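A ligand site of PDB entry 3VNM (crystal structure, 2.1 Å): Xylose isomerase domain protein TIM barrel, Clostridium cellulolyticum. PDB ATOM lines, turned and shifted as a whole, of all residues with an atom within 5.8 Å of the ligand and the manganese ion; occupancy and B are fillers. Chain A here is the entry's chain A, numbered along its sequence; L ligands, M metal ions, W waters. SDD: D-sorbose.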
ATOM      1  N   TYR A   6     -22.704  10.889  18.535  1.00  0.00           N
ATOM      2  CA  TYR A   6     -22.257  11.293  19.875  1.00  0.00           C
ATOM      3  C   TYR A   6     -22.514  12.827  19.997  1.00  0.00           C
ATOM      4  O   TYR A   6     -22.160  13.602  19.095  1.00  0.00           O
ATOM      5  CB  TYR A   6     -20.776  10.976  20.035  1.00  0.00           C
ATOM      6  CG  TYR A   6     -20.189  10.980  21.448  1.00  0.00           C
ATOM      7  CD1 TYR A   6     -20.980  10.728  22.580  1.00  0.00           C
ATOM      8  CD2 TYR A   6     -18.820  11.146  21.627  1.00  0.00           C
ATOM      9  CE1 TYR A   6     -20.417  10.652  23.865  1.00  0.00           C
ATOM     10  CE2 TYR A   6     -18.229  11.048  22.886  1.00  0.00           C
ATOM     11  CZ  TYR A   6     -19.042  10.813  24.003  1.00  0.00           C
ATOM     12  OH  TYR A   6     -18.432  10.747  25.236  1.00  0.00           O
ATOM     13  N   TRP A  14     -17.387  17.196  28.505  1.00  0.00           N
ATOM     14  CA  TRP A  14     -18.005  15.870  28.628  1.00  0.00           C
ATOM     15  C   TRP A  14     -19.342  15.860  29.380  1.00  0.00           C
ATOM     16  O   TRP A  14     -19.561  15.032  30.260  1.00  0.00           O
ATOM     17  CB  TRP A  14     -17.023  14.843  29.261  1.00  0.00           C
ATOM     18  CG  TRP A  14     -15.754  14.646  28.404  1.00  0.00           C
ATOM     19  CD1 TRP A  14     -14.464  14.917  28.779  1.00  0.00           C
ATOM     20  CD2 TRP A  14     -15.680  14.153  27.048  1.00  0.00           C
ATOM     21  NE1 TRP A  14     -13.582  14.628  27.745  1.00  0.00           N
ATOM     22  CE2 TRP A  14     -14.302  14.156  26.677  1.00  0.00           C
ATOM     23  CE3 TRP A  14     -16.644  13.730  26.114  1.00  0.00           C
ATOM     24  CZ2 TRP A  14     -13.866  13.734  25.408  1.00  0.00           C
ATOM     25  CZ3 TRP A  14     -16.200  13.311  24.838  1.00  0.00           C
ATOM     26  CH2 TRP A  14     -14.822  13.323  24.501  1.00  0.00           C
ATOM     27  N   GLU A  34     -25.870   9.289  21.490  1.00  0.00           N
ATOM     28  CA  GLU A  34     -24.952   8.691  22.483  1.00  0.00           C
ATOM     29  C   GLU A  34     -24.509   9.823  23.382  1.00  0.00           C
ATOM     30  O   GLU A  34     -24.153  10.880  22.885  1.00  0.00           O
ATOM     31  CB  GLU A  34     -23.746   8.016  21.802  1.00  0.00           C
ATOM     32  CG  GLU A  34     -22.709   7.458  22.810  1.00  0.00           C
ATOM     33  CD  GLU A  34     -21.939   6.205  22.269  1.00  0.00           C
ATOM     34  OE1 GLU A  34     -22.579   5.289  21.716  1.00  0.00           O
ATOM     35  OE2 GLU A  34     -20.711   6.165  22.416  1.00  0.00           O
ATOM     36  N   GLY A  65     -21.208   6.561  26.442  1.00  0.00           N
ATOM     37  CA  GLY A  65     -19.782   6.375  26.314  1.00  0.00           C
ATOM     38  C   GLY A  65     -19.105   6.914  27.570  1.00  0.00           C
ATOM     39  O   GLY A  65     -19.621   7.827  28.229  1.00  0.00           O
ATOM     40  N   HIS A  66     -17.938   6.368  27.913  1.00  0.00           N
ATOM     41  CA  HIS A  66     -17.208   6.893  29.069  1.00  0.00           C
ATOM     42  C   HIS A  66     -15.699   6.776  28.963  1.00  0.00           C
ATOM     43  O   HIS A  66     -15.171   5.729  28.594  1.00  0.00           O
ATOM     44  CB  HIS A  66     -17.632   6.198  30.371  1.00  0.00           C
ATOM     45  CG  HIS A  66     -17.169   6.916  31.595  1.00  0.00           C
ATOM     46  ND1 HIS A  66     -16.606   6.265  32.674  1.00  0.00           N
ATOM     47  CD2 HIS A  66     -17.215   8.223  31.927  1.00  0.00           C
ATOM     48  CE1 HIS A  66     -16.327   7.141  33.615  1.00  0.00           C
ATOM     49  NE2 HIS A  66     -16.690   8.340  33.182  1.00  0.00           N
ATOM     50  N   GLY A  67     -15.019   7.855  29.318  1.00  0.00           N
ATOM     51  CA  GLY A  67     -13.572   7.879  29.369  1.00  0.00           C
ATOM     52  C   GLY A  67     -13.311   7.851  30.874  1.00  0.00           C
ATOM     53  O   GLY A  67     -13.429   8.887  31.515  1.00  0.00           O
ATOM     54  N   GLY A 105     -20.094   2.058  26.648  1.00  0.00           N
ATOM     55  CA  GLY A 105     -18.894   1.669  25.948  1.00  0.00           C
ATOM     56  C   GLY A 105     -17.767   2.612  26.184  1.00  0.00           C
ATOM     57  O   GLY A 105     -17.976   3.708  26.748  1.00  0.00           O
ATOM     58  N   GLY A 106     -16.586   2.175  25.748  1.00  0.00           N
ATOM     59  CA  GLY A 106     -15.351   2.939  25.870  1.00  0.00           C
ATOM     60  C   GLY A 106     -14.222   2.135  26.519  1.00  0.00           C
ATOM     61  O   GLY A 106     -14.253   0.887  26.556  1.00  0.00           O
ATOM     62  N   ALA A 107     -13.239   2.822  27.075  1.00  0.00           N
ATOM     63  CA  ALA A 107     -12.089   2.166  27.703  1.00  0.00           C
ATOM     64  C   ALA A 107     -12.484   1.755  29.104  1.00  0.00           C
ATOM     65  O   ALA A 107     -11.799   2.091  30.054  1.00  0.00           O
ATOM     66  CB  ALA A 107     -10.900   3.140  27.779  1.00  0.00           C
ATOM     67  N   TRP A 112      -8.986   6.796  30.753  1.00  0.00           N
ATOM     68  CA  TRP A 112      -8.667   7.552  29.535  1.00  0.00           C
ATOM     69  C   TRP A 112      -8.939   9.038  29.752  1.00  0.00           C
ATOM     70  O   TRP A 112      -9.923   9.403  30.360  1.00  0.00           O
ATOM     71  CB  TRP A 112      -9.581   7.057  28.403  1.00  0.00           C
ATOM     72  CG  TRP A 112      -9.457   7.773  27.083  1.00  0.00           C
ATOM     73  CD1 TRP A 112      -8.652   7.419  26.021  1.00  0.00           C
ATOM     74  CD2 TRP A 112     -10.144   8.963  26.683  1.00  0.00           C
ATOM     75  NE1 TRP A 112      -8.791   8.328  24.991  1.00  0.00           N
ATOM     76  CE2 TRP A 112      -9.698   9.288  25.367  1.00  0.00           C
ATOM     77  CE3 TRP A 112     -11.083   9.794  27.307  1.00  0.00           C
ATOM     78  CZ2 TRP A 112     -10.170  10.406  24.667  1.00  0.00           C
ATOM     79  CZ3 TRP A 112     -11.556  10.926  26.597  1.00  0.00           C
ATOM     80  CH2 TRP A 112     -11.094  11.214  25.296  1.00  0.00           C
ATOM     81  N   GLU A 150     -13.999  -0.955  24.260  1.00  0.00           N
ATOM     82  CA  GLU A 150     -13.526  -0.363  23.007  1.00  0.00           C
ATOM     83  C   GLU A 150     -12.030  -0.526  22.739  1.00  0.00           C
ATOM     84  O   GLU A 150     -11.203  -0.175  23.572  1.00  0.00           O
ATOM     85  CB  GLU A 150     -13.898   1.146  22.936  1.00  0.00           C
ATOM     86  CG  GLU A 150     -13.380   1.854  21.687  1.00  0.00           C
ATOM     87  CD  GLU A 150     -13.766   3.376  21.637  1.00  0.00           C
ATOM     88  OE1 GLU A 150     -14.067   4.000  22.671  1.00  0.00           O
ATOM     89  OE2 GLU A 150     -13.759   3.956  20.554  1.00  0.00           O
ATOM     90  N   LEU A 152      -8.688   0.599  21.358  1.00  0.00           N
ATOM     91  CA  LEU A 152      -8.137   1.910  21.022  1.00  0.00           C
ATOM     92  C   LEU A 152      -6.733   1.894  20.452  1.00  0.00           C
ATOM     93  O   LEU A 152      -5.960   0.906  20.613  1.00  0.00           O
ATOM     94  CB  LEU A 152      -8.120   2.798  22.250  1.00  0.00           C
ATOM     95  CG  LEU A 152      -9.423   2.880  23.043  1.00  0.00           C
ATOM     96  CD1 LEU A 152      -9.108   3.494  24.359  1.00  0.00           C
ATOM     97  CD2 LEU A 152     -10.473   3.685  22.283  1.00  0.00           C
ATOM     98  N   ASN A 153      -6.343   3.013  19.825  1.00  0.00           N
ATOM     99  CA  ASN A 153      -5.011   3.050  19.281  1.00  0.00           C
ATOM    100  C   ASN A 153      -3.990   3.198  20.432  1.00  0.00           C
ATOM    101  O   ASN A 153      -4.304   3.595  21.577  1.00  0.00           O
ATOM    102  CB  ASN A 153      -4.862   4.175  18.239  1.00  0.00           C
ATOM    103  CG  ASN A 153      -4.948   5.570  18.842  1.00  0.00           C
ATOM    104  OD1 ASN A 153      -4.064   5.990  19.583  1.00  0.00           O
ATOM    105  ND2 ASN A 153      -6.022   6.302  18.519  1.00  0.00           N
ATOM    106  N   GLU A 156      -3.622   6.016  22.957  1.00  0.00           N
ATOM    107  CA  GLU A 156      -4.691   6.289  23.907  1.00  0.00           C
ATOM    108  C   GLU A 156      -4.949   5.169  24.904  1.00  0.00           C
ATOM    109  O   GLU A 156      -5.797   5.314  25.783  1.00  0.00           O
ATOM    110  CB  GLU A 156      -6.004   6.575  23.116  1.00  0.00           C
ATOM    111  CG  GLU A 156      -5.937   7.874  22.283  1.00  0.00           C
ATOM    112  CD  GLU A 156      -7.287   8.225  21.657  1.00  0.00           C
ATOM    113  OE1 GLU A 156      -8.295   8.320  22.405  1.00  0.00           O
ATOM    114  OE2 GLU A 156      -7.355   8.381  20.416  1.00  0.00           O
ATOM    115  N   MET A 181     -15.854  -3.663  21.139  1.00  0.00           N
ATOM    116  CA  MET A 181     -16.418  -2.509  20.451  1.00  0.00           C
ATOM    117  C   MET A 181     -15.307  -2.037  19.543  1.00  0.00           C
ATOM    118  O   MET A 181     -14.185  -1.914  19.987  1.00  0.00           O
ATOM    119  CB  MET A 181     -16.765  -1.464  21.499  1.00  0.00           C
ATOM    120  CG  MET A 181     -17.105  -0.051  20.987  1.00  0.00           C
ATOM    121  SD  MET A 181     -17.612   1.004  22.360  1.00  0.00           S
ATOM    122  CE  MET A 181     -17.399   2.708  21.543  1.00  0.00           C
ATOM    123  N   ASP A 183     -13.889   0.837  16.433  1.00  0.00           N
ATOM    124  CA  ASP A 183     -14.022   2.230  16.067  1.00  0.00           C
ATOM    125  C   ASP A 183     -13.152   2.455  14.814  1.00  0.00           C
ATOM    126  O   ASP A 183     -11.952   2.267  14.844  1.00  0.00           O
ATOM    127  CB  ASP A 183     -13.566   3.075  17.265  1.00  0.00           C
ATOM    128  CG  ASP A 183     -13.474   4.593  16.978  1.00  0.00           C
ATOM    129  OD1 ASP A 183     -13.158   5.023  15.855  1.00  0.00           O
ATOM    130  OD2 ASP A 183     -13.657   5.365  17.940  1.00  0.00           O
ATOM    131  N   PHE A 185     -11.888   4.971  13.428  1.00  0.00           N
ATOM    132  CA  PHE A 185     -10.731   5.831  13.630  1.00  0.00           C
ATOM    133  C   PHE A 185      -9.499   5.104  14.279  1.00  0.00           C
ATOM    134  O   PHE A 185      -8.323   5.416  13.957  1.00  0.00           O
ATOM    135  CB  PHE A 185     -11.120   7.045  14.517  1.00  0.00           C
ATOM    136  CG  PHE A 185      -9.937   7.842  15.050  1.00  0.00           C
ATOM    137  CD1 PHE A 185      -9.155   8.637  14.203  1.00  0.00           C
ATOM    138  CD2 PHE A 185      -9.584   7.747  16.371  1.00  0.00           C
ATOM    139  CE1 PHE A 185      -8.041   9.311  14.663  1.00  0.00           C
ATOM    140  CE2 PHE A 185      -8.467   8.406  16.870  1.00  0.00           C
ATOM    141  CZ  PHE A 185      -7.673   9.211  15.997  1.00  0.00           C
ATOM    142  N   HIS A 186      -9.782   4.165  15.196  1.00  0.00           N
ATOM    143  CA  HIS A 186      -8.711   3.438  15.893  1.00  0.00           C
ATOM    144  C   HIS A 186      -8.212   2.252  15.078  1.00  0.00           C
ATOM    145  O   HIS A 186      -7.033   1.911  15.143  1.00  0.00           O
ATOM    146  CB  HIS A 186      -9.181   2.946  17.276  1.00  0.00           C
ATOM    147  CG  HIS A 186      -9.413   4.062  18.260  1.00  0.00           C
ATOM    148  ND1 HIS A 186      -8.410   4.923  18.646  1.00  0.00           N
ATOM    149  CD2 HIS A 186     -10.550   4.495  18.850  1.00  0.00           C
ATOM    150  CE1 HIS A 186      -8.919   5.846  19.445  1.00  0.00           C
ATOM    151  NE2 HIS A 186     -10.213   5.613  19.584  1.00  0.00           N
ATOM    152  N   HIS A 209     -18.256   2.537  16.547  1.00  0.00           N
ATOM    153  CA  HIS A 209     -18.097   4.001  16.432  1.00  0.00           C
ATOM    154  C   HIS A 209     -17.525   4.282  15.045  1.00  0.00           C
ATOM    155  O   HIS A 209     -16.633   3.546  14.559  1.00  0.00           O
ATOM    156  CB  HIS A 209     -17.053   4.554  17.366  1.00  0.00           C
ATOM    157  CG  HIS A 209     -17.550   4.960  18.701  1.00  0.00           C
ATOM    158  ND1 HIS A 209     -16.698   5.424  19.688  1.00  0.00           N
ATOM    159  CD2 HIS A 209     -18.790   4.934  19.250  1.00  0.00           C
ATOM    160  CE1 HIS A 209     -17.397   5.649  20.785  1.00  0.00           C
ATOM    161  NE2 HIS A 209     -18.665   5.357  20.551  1.00  0.00           N
ATOM    162  N   ARG A 215     -11.118  12.022  12.067  1.00  0.00           N
ATOM    163  CA  ARG A 215     -12.303  12.232  12.925  1.00  0.00           C
ATOM    164  C   ARG A 215     -13.377  13.150  12.346  1.00  0.00           C
ATOM    165  O   ARG A 215     -14.186  13.723  13.091  1.00  0.00           O
ATOM    166  CB  ARG A 215     -11.876  12.758  14.283  1.00  0.00           C
ATOM    167  CG  ARG A 215     -10.918  11.820  15.074  1.00  0.00           C
ATOM    168  CD  ARG A 215     -11.742  10.800  15.889  1.00  0.00           C
ATOM    169  NE  ARG A 215     -11.123  10.713  17.151  1.00  0.00           N
ATOM    170  CZ  ARG A 215     -11.459   9.918  18.135  1.00  0.00           C
ATOM    171  NH1 ARG A 215     -12.483   9.065  18.033  1.00  0.00           N
ATOM    172  NH2 ARG A 215     -10.675   9.935  19.221  1.00  0.00           N
ATOM    173  N   GLU A 244     -18.878   9.375  15.659  1.00  0.00           N
ATOM    174  CA  GLU A 244     -18.277  10.138  16.717  1.00  0.00           C
ATOM    175  C   GLU A 244     -17.339  11.215  16.121  1.00  0.00           C
ATOM    176  O   GLU A 244     -16.130  11.245  16.364  1.00  0.00           O
ATOM    177  CB  GLU A 244     -17.526   9.115  17.550  1.00  0.00           C
ATOM    178  CG  GLU A 244     -16.969   9.600  18.770  1.00  0.00           C
ATOM    179  CD  GLU A 244     -16.178   8.479  19.471  1.00  0.00           C
ATOM    180  OE1 GLU A 244     -15.425   7.768  18.775  1.00  0.00           O
ATOM    181  OE2 GLU A 244     -16.319   8.360  20.686  1.00  0.00           O
ATOM    182  N   PHE A 246     -15.303  14.674  15.670  1.00  0.00           N
ATOM    183  CA  PHE A 246     -14.715  15.685  16.529  1.00  0.00           C
ATOM    184  C   PHE A 246     -14.029  16.644  15.586  1.00  0.00           C
ATOM    185  O   PHE A 246     -12.892  16.410  15.178  1.00  0.00           O
ATOM    186  CB  PHE A 246     -13.671  15.084  17.482  1.00  0.00           C
ATOM    187  CG  PHE A 246     -14.260  14.184  18.556  1.00  0.00           C
ATOM    188  CD1 PHE A 246     -14.966  14.719  19.628  1.00  0.00           C
ATOM    189  CD2 PHE A 246     -14.136  12.799  18.455  1.00  0.00           C
ATOM    190  CE1 PHE A 246     -15.548  13.883  20.620  1.00  0.00           C
ATOM    191  CE2 PHE A 246     -14.725  11.938  19.430  1.00  0.00           C
ATOM    192  CZ  PHE A 246     -15.424  12.475  20.495  1.00  0.00           C
ATOM    193  N   ILE A 257      -9.275  14.891  22.796  1.00  0.00           N
ATOM    194  CA  ILE A 257      -9.276  14.335  21.459  1.00  0.00           C
ATOM    195  C   ILE A 257      -8.083  14.849  20.644  1.00  0.00           C
ATOM    196  O   ILE A 257      -7.766  14.328  19.596  1.00  0.00           O
ATOM    197  CB  ILE A 257     -10.630  14.688  20.742  1.00  0.00           C
ATOM    198  CG1 ILE A 257     -11.828  14.157  21.573  1.00  0.00           C
ATOM    199  CG2 ILE A 257     -10.701  14.083  19.361  1.00  0.00           C
ATOM    200  CD1 ILE A 257     -11.839  12.627  21.760  1.00  0.00           C
HETATM  201  C1  SDD L   1     -11.718   8.190  22.011  1.00  0.00           C
HETATM  202  O1  SDD L   1     -10.533   7.951  21.256  1.00  0.00           O
HETATM  203  C2  SDD L   1     -12.791   7.120  21.746  1.00  0.00           C
HETATM  204  O2  SDD L   1     -13.072   6.736  20.615  1.00  0.00           O
HETATM  205  C3  SDD L   1     -13.845   7.015  22.845  1.00  0.00           C
HETATM  206  O3  SDD L   1     -14.996   6.400  22.259  1.00  0.00           O
HETATM  207  C4  SDD L   1     -14.194   8.432  23.292  1.00  0.00           C
HETATM  208  O4  SDD L   1     -14.427   9.240  22.130  1.00  0.00           O
HETATM  209  C5  SDD L   1     -15.423   8.403  24.211  1.00  0.00           C
HETATM  210  O5  SDD L   1     -15.915   9.729  24.412  1.00  0.00           O
HETATM  211  C6  SDD L   1     -15.033   7.813  25.568  1.00  0.00           C
HETATM  212  O6  SDD L   1     -14.587   6.466  25.415  1.00  0.00           O
HETATM  213 MN    MN M   1     -14.682   5.818  19.813  1.00  0.00          MN
HETATM  214  O   HOH W   1     -14.772  10.865  27.423  1.00  0.00           O
HETATM  215  O   HOH W   2     -18.519   7.755  23.096  1.00  0.00           O
HETATM  216  O   HOH W   3     -16.857   5.475  24.516  1.00  0.00           O
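The backbone carbonyl oxygen of His 66 lies within hydrogen-bond range of an oxygen (O6) of the ligand, 3.3 Å away.
The guanidinium group of Arg 215 is in hydrogen-bond range of an oxygen (O1) of the ligand (2.8 Å).
The side-chain carboxylate (OE1) of Glu 156 is in hydrogen-bond range of an oxygen (O1) of the ligand.
A ring nitrogen (NE2) of His 186 is in hydrogen-bond range of an oxygen (O1) of the ligand (2.9 Å).
An oxygen (O5) of the ligand sits at hydrogen-bond distance from the side-chain hydroxyl (OH) of Tyr 6, at 2.8 Å.
Along chain A the residues within 4 Å of the manganese ion span positions 150 to 244.
Water W3 lies within hydrogen-bond range of an oxygen (O6) of the ligand and the backbone carbonyl oxygen (O) of Gly 105.
Water W2 lies within hydrogen-bond range of OE2 of Glu 34 (2.8 Å), OE2 of Glu 244 (3.3 Å) and NE2 of His 209 (3.5 Å).
The manganese ion is bound by an oxygen (O2) of the ligand, a ring nitrogen (ND1) of His 209, the side-chain carboxylate (OD2) of Asp 183, the side-chain carboxylate (OE2) of Glu 150, the side-chain carboxylate (OE1) of Glu 244 and an oxygen (O3) of the ligand.
The backbone carbonyl oxygen (O) of Arg 215 is in hydrogen-bond range of the backbone NH (N) of Phe 246 (3.0 Å).
NH1 of Arg 215 lies close to OD2 of Asp 183 (3.9 Å).
NE2 of His 209 lies within hydrogen-bond range of OE2 of Glu 34 (2.9 Å).
The side-chain carboxylate of Glu 156 sits at hydrogen-bond distance from the side-chain amide nitrogen of Asn 153 (3.1 Å).
ND2 of Asn 153 is in hydrogen-bond range of ND1 of His 186, at 2.8 Å.
N of Glu 150 sits at hydrogen-bond distance from O of Gly 106, 3.0 Å away.
NH2 of Arg 215 is in salt-bridge range of OE2 of Glu 156.
The indole nitrogen (NE1) of Trp 112 sits at hydrogen-bond distance from the side-chain carboxylate (OE1) of Glu 156, at 2.6 Å.
Trp 14 touches the ligand.
Gly 67 touches the ligand.
Gly 106 touches the ligand (CA to O6, 3.6 Å).
Trp 112 touches the ligand (CZ2 to C1, 3.8 Å).
CZ of Phe 246 touches O4 of the ligand, at 3.8 Å.
Hydrophobic or aromatic side chains within 4 Å of the ligand: Tyr 6, Trp 14, Trp 112, His 186, His 209 and Phe 246.
Within 4 Å of the ligand: Tyr 6, Trp 14, His 66, Gly 67, Gly 106, Trp 112, Glu 150, Glu 156, Asp 183, His 186, His 209, Arg 215, Glu 244 and Phe 246.
The nearest printed residue that does not touch the ligand is Leu 152 (4.2 Å).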
